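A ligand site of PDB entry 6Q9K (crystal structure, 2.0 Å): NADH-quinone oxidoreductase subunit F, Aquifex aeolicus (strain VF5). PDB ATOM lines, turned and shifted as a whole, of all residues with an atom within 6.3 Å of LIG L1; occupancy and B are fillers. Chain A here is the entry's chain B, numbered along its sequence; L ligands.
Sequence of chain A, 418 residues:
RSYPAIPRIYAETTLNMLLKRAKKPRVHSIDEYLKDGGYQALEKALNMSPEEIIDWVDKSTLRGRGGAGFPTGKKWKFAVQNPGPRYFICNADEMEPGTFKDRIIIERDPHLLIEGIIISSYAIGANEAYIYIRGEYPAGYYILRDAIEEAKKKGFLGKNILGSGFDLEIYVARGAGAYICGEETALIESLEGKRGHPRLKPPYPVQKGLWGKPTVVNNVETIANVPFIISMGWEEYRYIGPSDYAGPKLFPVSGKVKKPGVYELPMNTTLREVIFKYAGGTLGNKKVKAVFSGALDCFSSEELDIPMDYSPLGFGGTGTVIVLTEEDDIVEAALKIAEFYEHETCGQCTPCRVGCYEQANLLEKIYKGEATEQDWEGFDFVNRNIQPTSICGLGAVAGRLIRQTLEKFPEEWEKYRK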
ATOM      1  N   ILE A 180      -8.796  25.968   6.337  1.00  0.00           N
ATOM      2  CA  ILE A 180      -9.593  24.883   6.976  1.00  0.00           C
ATOM      3  C   ILE A 180     -11.083  25.149   6.762  1.00  0.00           C
ATOM      4  O   ILE A 180     -11.843  24.183   6.821  1.00  0.00           O
ATOM      5  CB  ILE A 180      -9.244  24.730   8.464  1.00  0.00           C
ATOM      6  CG1 ILE A 180      -9.805  23.417   9.037  1.00  0.00           C
ATOM      7  CG2 ILE A 180      -9.709  25.932   9.280  1.00  0.00           C
ATOM      8  CD1 ILE A 180      -9.345  22.186   8.282  1.00  0.00           C
ATOM      9  N   GLY A 196     -13.649  28.026  12.502  1.00  0.00           N
ATOM     10  CA  GLY A 196     -13.616  26.918  11.517  1.00  0.00           C
ATOM     11  C   GLY A 196     -12.953  25.672  12.077  1.00  0.00           C
ATOM     12  O   GLY A 196     -11.815  25.378  11.665  1.00  0.00           O
ATOM     13  N   HIS A 197     -13.631  24.989  13.011  1.00  0.00           N
ATOM     14  CA  HIS A 197     -13.230  23.675  13.580  1.00  0.00           C
ATOM     15  C   HIS A 197     -14.040  22.572  12.891  1.00  0.00           C
ATOM     16  O   HIS A 197     -15.251  22.495  13.067  1.00  0.00           O
ATOM     17  CB  HIS A 197     -13.401  23.656  15.088  1.00  0.00           C
ATOM     18  CG  HIS A 197     -12.428  24.530  15.798  1.00  0.00           C
ATOM     19  ND1 HIS A 197     -12.573  24.860  17.131  1.00  0.00           N
ATOM     20  CD2 HIS A 197     -11.310  25.146  15.371  1.00  0.00           C
ATOM     21  CE1 HIS A 197     -11.573  25.632  17.496  1.00  0.00           C
ATOM     22  NE2 HIS A 197     -10.785  25.832  16.436  1.00  0.00           N
ATOM     23  N   PRO A 198     -13.388  21.713  12.081  1.00  0.00           N
ATOM     24  CA  PRO A 198     -14.046  20.523  11.536  1.00  0.00           C
ATOM     25  C   PRO A 198     -14.706  19.684  12.626  1.00  0.00           C
ATOM     26  O   PRO A 198     -14.201  19.658  13.749  1.00  0.00           O
ATOM     27  CB  PRO A 198     -12.905  19.750  10.877  1.00  0.00           C
ATOM     28  CG  PRO A 198     -11.890  20.820  10.504  1.00  0.00           C
ATOM     29  CD  PRO A 198     -11.998  21.852  11.609  1.00  0.00           C
ATOM     30  N   ARG A 199     -15.821  19.045  12.266  1.00  0.00           N
ATOM     31  CA  ARG A 199     -16.591  18.076  13.094  1.00  0.00           C
ATOM     32  C   ARG A 199     -16.143  16.648  12.756  1.00  0.00           C
ATOM     33  O   ARG A 199     -15.861  16.371  11.554  1.00  0.00           O
ATOM     34  CB  ARG A 199     -18.084  18.178  12.768  1.00  0.00           C
ATOM     35  CG  ARG A 199     -18.699  19.547  13.031  1.00  0.00           C
ATOM     36  CD  ARG A 199     -20.133  19.560  12.545  1.00  0.00           C
ATOM     37  NE  ARG A 199     -20.798  20.843  12.755  1.00  0.00           N
ATOM     38  CZ  ARG A 199     -22.021  21.149  12.326  1.00  0.00           C
ATOM     39  NH1 ARG A 199     -22.530  22.343  12.586  1.00  0.00           N
ATOM     40  NH2 ARG A 199     -22.741  20.258  11.650  1.00  0.00           N
ATOM     41  N   GLU A 344      -2.028  26.529   8.645  1.00  0.00           N
ATOM     42  CA  GLU A 344      -3.484  26.246   8.431  1.00  0.00           C
ATOM     43  C   GLU A 344      -4.097  25.179   9.363  1.00  0.00           C
ATOM     44  O   GLU A 344      -5.331  25.146   9.438  1.00  0.00           O
ATOM     45  CB  GLU A 344      -3.742  25.856   6.976  1.00  0.00           C
ATOM     46  CG  GLU A 344      -3.333  26.939   6.000  1.00  0.00           C
ATOM     47  CD  GLU A 344      -3.916  28.332   6.213  1.00  0.00           C
ATOM     48  OE1 GLU A 344      -5.038  28.445   6.794  1.00  0.00           O
ATOM     49  OE2 GLU A 344      -3.253  29.309   5.811  1.00  0.00           O
ATOM     50  N   THR A 345      -3.334  24.334  10.065  1.00  0.00           N
ATOM     51  CA  THR A 345      -3.940  23.363  11.028  1.00  0.00           C
ATOM     52  C   THR A 345      -4.766  24.159  12.041  1.00  0.00           C
ATOM     53  O   THR A 345      -4.306  25.219  12.476  1.00  0.00           O
ATOM     54  CB  THR A 345      -2.894  22.476  11.731  1.00  0.00           C
ATOM     55  OG1 THR A 345      -3.576  21.691  12.723  1.00  0.00           O
ATOM     56  CG2 THR A 345      -1.789  23.276  12.380  1.00  0.00           C
ATOM     57  N   CYS A 346      -5.973  23.703  12.379  1.00  0.00           N
ATOM     58  CA  CYS A 346      -6.877  24.394  13.343  1.00  0.00           C
ATOM     59  C   CYS A 346      -6.503  24.024  14.779  1.00  0.00           C
ATOM     60  O   CYS A 346      -6.919  24.759  15.697  1.00  0.00           O
ATOM     61  CB  CYS A 346      -8.343  24.095  13.048  1.00  0.00           C
ATOM     62  SG  CYS A 346      -8.895  22.442  13.565  1.00  0.00           S
ATOM     63  N   GLY A 347      -5.735  22.937  14.983  1.00  0.00           N
ATOM     64  CA  GLY A 347      -5.146  22.585  16.287  1.00  0.00           C
ATOM     65  C   GLY A 347      -6.032  21.725  17.192  1.00  0.00           C
ATOM     66  O   GLY A 347      -5.591  21.414  18.300  1.00  0.00           O
ATOM     67  N   GLN A 348      -7.209  21.299  16.739  1.00  0.00           N
ATOM     68  CA  GLN A 348      -8.109  20.427  17.555  1.00  0.00           C
ATOM     69  C   GLN A 348      -7.432  19.090  17.870  1.00  0.00           C
ATOM     70  O   GLN A 348      -7.643  18.577  18.994  1.00  0.00           O
ATOM     71  CB  GLN A 348      -9.401  20.113  16.812  1.00  0.00           C
ATOM     72  CG  GLN A 348     -10.431  21.216  16.842  1.00  0.00           C
ATOM     73  CD  GLN A 348     -11.724  20.690  16.301  1.00  0.00           C
ATOM     74  OE1 GLN A 348     -12.638  20.353  17.058  1.00  0.00           O
ATOM     75  NE2 GLN A 348     -11.803  20.530  14.975  1.00  0.00           N
ATOM     76  N   CYS A 349      -6.725  18.512  16.893  1.00  0.00           N
ATOM     77  CA  CYS A 349      -6.109  17.162  17.002  1.00  0.00           C
ATOM     78  C   CYS A 349      -4.610  17.329  17.305  1.00  0.00           C
ATOM     79  O   CYS A 349      -3.961  18.131  16.631  1.00  0.00           O
ATOM     80  CB  CYS A 349      -6.333  16.344  15.726  1.00  0.00           C
ATOM     81  SG  CYS A 349      -7.999  16.508  15.015  1.00  0.00           S
ATOM     82  N   THR A 350      -4.094  16.608  18.295  1.00  0.00           N
ATOM     83  CA  THR A 350      -2.722  16.848  18.828  1.00  0.00           C
ATOM     84  C   THR A 350      -1.676  16.534  17.740  1.00  0.00           C
ATOM     85  O   THR A 350      -0.861  17.398  17.428  1.00  0.00           O
ATOM     86  CB  THR A 350      -2.535  16.139  20.181  1.00  0.00           C
ATOM     87  OG1 THR A 350      -3.307  16.888  21.130  1.00  0.00           O
ATOM     88  CG2 THR A 350      -1.081  16.052  20.598  1.00  0.00           C
ATOM     89  N   CYS A 352      -1.806  16.476  14.562  1.00  0.00           N
ATOM     90  CA  CYS A 352      -1.918  17.509  13.495  1.00  0.00           C
ATOM     91  C   CYS A 352      -1.343  18.847  13.990  1.00  0.00           C
ATOM     92  O   CYS A 352      -0.521  19.435  13.258  1.00  0.00           O
ATOM     93  CB  CYS A 352      -3.366  17.686  13.027  1.00  0.00           C
ATOM     94  SG  CYS A 352      -3.530  18.858  11.666  1.00  0.00           S
ATOM     95  N   ARG A 353      -1.769  19.312  15.160  1.00  0.00           N
ATOM     96  CA  ARG A 353      -1.311  20.605  15.758  1.00  0.00           C
ATOM     97  C   ARG A 353       0.218  20.618  15.846  1.00  0.00           C
ATOM     98  O   ARG A 353       0.844  21.572  15.326  1.00  0.00           O
ATOM     99  CB  ARG A 353      -1.947  20.796  17.141  1.00  0.00           C
ATOM    100  CG  ARG A 353      -1.620  22.130  17.798  1.00  0.00           C
ATOM    101  CD  ARG A 353      -2.400  22.308  19.089  1.00  0.00           C
ATOM    102  NE  ARG A 353      -1.998  21.343  20.111  1.00  0.00           N
ATOM    103  CZ  ARG A 353      -2.699  20.297  20.539  1.00  0.00           C
ATOM    104  NH1 ARG A 353      -3.910  20.031  20.054  1.00  0.00           N
ATOM    105  NH2 ARG A 353      -2.172  19.521  21.470  1.00  0.00           N
ATOM    106  N   CYS A 356       2.264  19.408  12.046  1.00  0.00           N
ATOM    107  CA  CYS A 356       2.315  20.463  11.009  1.00  0.00           C
ATOM    108  C   CYS A 356       3.370  21.519  11.392  1.00  0.00           C
ATOM    109  O   CYS A 356       4.141  21.947  10.512  1.00  0.00           O
ATOM    110  CB  CYS A 356       0.954  21.129  10.800  1.00  0.00           C
ATOM    111  SG  CYS A 356      -0.245  20.034  10.008  1.00  0.00           S
ATOM    112  N   ILE A 386       1.556  12.733  11.424  1.00  0.00           N
ATOM    113  CA  ILE A 386       0.609  13.885  11.480  1.00  0.00           C
ATOM    114  C   ILE A 386      -0.826  13.350  11.490  1.00  0.00           C
ATOM    115  O   ILE A 386      -1.674  13.956  12.181  1.00  0.00           O
ATOM    116  CB  ILE A 386       0.841  14.894  10.349  1.00  0.00           C
ATOM    117  CG1 ILE A 386       2.268  15.460  10.377  1.00  0.00           C
ATOM    118  CG2 ILE A 386      -0.206  15.999  10.444  1.00  0.00           C
ATOM    119  CD1 ILE A 386       2.669  16.245   9.152  1.00  0.00           C
ATOM    120  N   THR A 389      -5.305  10.063  14.778  1.00  0.00           N
ATOM    121  CA  THR A 389      -6.450  10.676  15.509  1.00  0.00           C
ATOM    122  C   THR A 389      -7.059  11.885  14.788  1.00  0.00           C
ATOM    123  O   THR A 389      -8.000  12.474  15.354  1.00  0.00           O
ATOM    124  CB  THR A 389      -6.066  11.099  16.933  1.00  0.00           C
ATOM    125  OG1 THR A 389      -5.393  12.360  16.889  1.00  0.00           O
ATOM    126  CG2 THR A 389      -5.217  10.059  17.632  1.00  0.00           C
ATOM    127  N   SER A 390      -6.589  12.228  13.584  1.00  0.00           N
ATOM    128  CA  SER A 390      -7.080  13.397  12.798  1.00  0.00           C
ATOM    129  C   SER A 390      -8.578  13.208  12.497  1.00  0.00           C
ATOM    130  O   SER A 390      -8.959  12.069  12.160  1.00  0.00           O
ATOM    131  CB  SER A 390      -6.291  13.600  11.533  1.00  0.00           C
ATOM    132  OG  SER A 390      -6.379  12.471  10.673  1.00  0.00           O
ATOM    133  N   ILE A 391      -9.370  14.280  12.574  1.00  0.00           N
ATOM    134  CA  ILE A 391     -10.835  14.219  12.292  1.00  0.00           C
ATOM    135  C   ILE A 391     -11.141  14.918  10.964  1.00  0.00           C
ATOM    136  O   ILE A 391     -12.335  15.065  10.662  1.00  0.00           O
ATOM    137  CB  ILE A 391     -11.664  14.763  13.469  1.00  0.00           C
ATOM    138  CG1 ILE A 391     -11.419  16.249  13.735  1.00  0.00           C
ATOM    139  CG2 ILE A 391     -11.433  13.924  14.724  1.00  0.00           C
ATOM    140  CD1 ILE A 391     -12.213  16.779  14.915  1.00  0.00           C
ATOM    141  N   CYS A 392     -10.131  15.326  10.191  1.00  0.00           N
ATOM    142  CA  CYS A 392     -10.358  15.865   8.819  1.00  0.00           C
ATOM    143  C   CYS A 392      -9.159  15.612   7.904  1.00  0.00           C
ATOM    144  O   CYS A 392      -8.090  15.163   8.383  1.00  0.00           O
ATOM    145  CB  CYS A 392     -10.736  17.351   8.861  1.00  0.00           C
ATOM    146  SG  CYS A 392      -9.340  18.478   8.687  1.00  0.00           S
ATOM    147  N   GLY A 393      -9.346  15.889   6.617  1.00  0.00           N
ATOM    148  CA  GLY A 393      -8.394  15.589   5.541  1.00  0.00           C
ATOM    149  C   GLY A 393      -7.065  16.328   5.672  1.00  0.00           C
ATOM    150  O   GLY A 393      -6.107  15.858   5.060  1.00  0.00           O
ATOM    151  N   LEU A 394      -7.005  17.463   6.386  1.00  0.00           N
ATOM    152  CA  LEU A 394      -5.763  18.277   6.501  1.00  0.00           C
ATOM    153  C   LEU A 394      -4.705  17.441   7.239  1.00  0.00           C
ATOM    154  O   LEU A 394      -3.615  17.232   6.672  1.00  0.00           O
ATOM    155  CB  LEU A 394      -6.034  19.599   7.229  1.00  0.00           C
ATOM    156  CG  LEU A 394      -4.918  20.639   7.123  1.00  0.00           C
ATOM    157  CD1 LEU A 394      -5.447  22.048   7.340  1.00  0.00           C
ATOM    158  CD2 LEU A 394      -3.782  20.341   8.107  1.00  0.00           C
ATOM    159  N   GLY A 395      -5.034  16.971   8.452  1.00  0.00           N
ATOM    160  CA  GLY A 395      -4.193  16.031   9.201  1.00  0.00           C
ATOM    161  C   GLY A 395      -3.862  14.783   8.393  1.00  0.00           C
ATOM    162  O   GLY A 395      -2.718  14.328   8.449  1.00  0.00           O
ATOM    163  N   ALA A 396      -4.839  14.258   7.648  1.00  0.00           N
ATOM    164  CA  ALA A 396      -4.688  13.019   6.851  1.00  0.00           C
ATOM    165  C   ALA A 396      -3.597  13.176   5.761  1.00  0.00           C
ATOM    166  O   ALA A 396      -2.983  12.161   5.415  1.00  0.00           O
ATOM    167  CB  ALA A 396      -6.020  12.634   6.239  1.00  0.00           C
HETATM  168 FE1  LIG L   1      -7.921  20.598  12.706  1.00  0.00          FE
HETATM  169 FE2  LIG L   1      -5.808  19.127  11.748  1.00  0.00          FE
HETATM  170 FE3  LIG L   1      -8.319  18.787  10.722  1.00  0.00          FE
HETATM  171 FE4  LIG L   1      -7.706  17.968  13.283  1.00  0.00          FE
HETATM  172  S1  LIG L   1      -6.820  17.151  11.333  1.00  0.00           S
HETATM  173  S2  LIG L   1      -9.595  19.059  12.615  1.00  0.00           S
HETATM  174  S3  LIG L   1      -6.297  19.592  13.952  1.00  0.00           S
HETATM  175  S4  LIG L   1      -7.040  20.679  10.615  1.00  0.00           S
HETATM  176  N1  LG2 L   2     -13.725  21.782  -1.249  1.00  0.00           N
HETATM  177  C1  LG2 L   2     -14.013  22.893  -1.994  1.00  0.00           C
HETATM  178  O1  LG2 L   2     -14.923  22.880  -2.842  1.00  0.00           O
HETATM  179  N2  LG2 L   2     -13.299  24.074  -1.763  1.00  0.00           N
HETATM  180  C2  LG2 L   2     -12.330  24.266  -0.798  1.00  0.00           C
HETATM  181  O2  LG2 L   2     -11.770  25.352  -0.695  1.00  0.00           O
HETATM  182  C3  LG2 L   2     -12.063  23.071   0.018  1.00  0.00           C
HETATM  183  N3  LG2 L   2     -11.202  23.172   0.997  1.00  0.00           N
HETATM  184  C4  LG2 L   2     -10.963  22.042   1.780  1.00  0.00           C
HETATM  185  C5  LG2 L   2     -10.026  22.121   2.810  1.00  0.00           C
HETATM  186  C6  LG2 L   2      -9.699  21.003   3.570  1.00  0.00           C
HETATM  187  C7  LG2 L   2      -8.663  21.118   4.662  1.00  0.00           C
HETATM  188  C8  LG2 L   2     -10.339  19.775   3.303  1.00  0.00           C
HETATM  189  C9  LG2 L   2      -9.965  18.520   4.052  1.00  0.00           C
HETATM  190  C10 LG2 L   2     -11.304  19.707   2.311  1.00  0.00           C
HETATM  191  C11 LG2 L   2     -11.617  20.820   1.532  1.00  0.00           C
HETATM  192  N4  LG2 L   2     -12.568  20.772   0.472  1.00  0.00           N
HETATM  193  C12 LG2 L   2     -12.809  21.886  -0.292  1.00  0.00           C
HETATM  194  C13 LG2 L   2     -13.395  19.581   0.230  1.00  0.00           C
HETATM  195  C14 LG2 L   2     -14.745  19.680   0.938  1.00  0.00           C
HETATM  196  O3  LG2 L   2     -14.628  19.249   2.293  1.00  0.00           O
HETATM  197  C15 LG2 L   2     -15.804  18.839   0.209  1.00  0.00           C
HETATM  198  O4  LG2 L   2     -15.279  17.558  -0.077  1.00  0.00           O
HETATM  199  C16 LG2 L   2     -16.321  19.450  -1.093  1.00  0.00           C
HETATM  200  O5  LG2 L   2     -16.573  20.850  -0.941  1.00  0.00           O
HETATM  201  C17 LG2 L   2     -17.572  18.738  -1.557  1.00  0.00           C
HETATM  202  O6  LG2 L   2     -17.919  19.231  -2.859  1.00  0.00           O
HETATM  203  P1  LG2 L   2     -17.703  18.337  -4.157  1.00  0.00           P
HETATM  204  O7  LG2 L   2     -16.241  18.295  -4.506  1.00  0.00           O
HETATM  205  O8  LG2 L   2     -18.268  16.930  -3.846  1.00  0.00           O
HETATM  206  O9  LG2 L   2     -18.609  18.970  -5.215  1.00  0.00           O
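Residues that only touch LIG L1: Ile 180, Pro 198, Ser 390, Ile 391 and Leu 394. Hydrophobic or aromatic side chains within 4 Å of LIG L1: Ile 180, Pro 198, Ile 391 and Leu 394. Within 4 Å of LIG L1: Ile 180, Pro 198, Thr 345, Cys 346, Gly 347, Gln 348, Cys 349, Cys 352, Ser 390, Ile 391, Cys 392, Leu 394 and Gly 395. Along chain A the residues within 4 Å of LIG L1 span positions 180 to 395. The nearest printed residue that does not touch LIG L1 is Arg 353 (4.7 Å).
The side-chain hydroxyl of Thr 345 lies close to a sulfur (S3) of LIG L1 (3.6 Å). A sulfur (S4) of LIG L1 sits close to the backbone NH (N) of Cys 346 (3.7 Å). A sulfur (S3) of LIG L1 lies close to the backbone NH (N) of Gly 347 (3.5 Å). The side-chain sulfur of Cys 352 is bound to an iron atom (FE2) of LIG L1 (2.3 Å). A sulfur (S1) of LIG L1 lies close to the backbone NH of Gly 395. The side-chain sulfur of Cys 349 binds an iron atom (FE4) of LIG L1. An iron atom (FE1) of LIG L1 is bound by the side-chain sulfur of Cys 346 (2.3 Å). The backbone NH (N) of Cys 349 lies close to a sulfur (S3) of LIG L1, 3.2 Å away. NE2 of Gln 348 sits close to S2 of LIG L1, at 3.6 Å. FE3 of LIG L1 is bound by SG of Cys 392 (2.3 Å). The backbone NH (N) of Gln 348 sits close to a sulfur (S3) of LIG L1 (3.4 Å).
The side-chain hydroxyl of Thr 345 sits close to the backbone NH of Gly 347. The side-chain sulfur of Cys 349 sits close to the backbone NH of Ile 391, 3.6 Å away. The backbone carbonyl oxygen (O) of Gly 347 lies within hydrogen-bond range of the guanidinium group (NH1) of Arg 353. The side-chain sulfur of Cys 346 sits close to the side-chain amide nitrogen of Gln 348. The side-chain sulfur (SG) of Cys 392 sits close to the backbone NH (N) of Leu 394 (3.4 Å). The backbone NH (N) of Cys 352 sits at hydrogen-bond distance from the backbone carbonyl oxygen (O) of Ile 386. NE2 of Gln 348 lies within hydrogen-bond range of O of Pro 198 (2.8 Å). The side-chain hydroxyl (OG1) of Thr 345 sits close to the side-chain sulfur (SG) of Cys 352 (3.0 Å).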
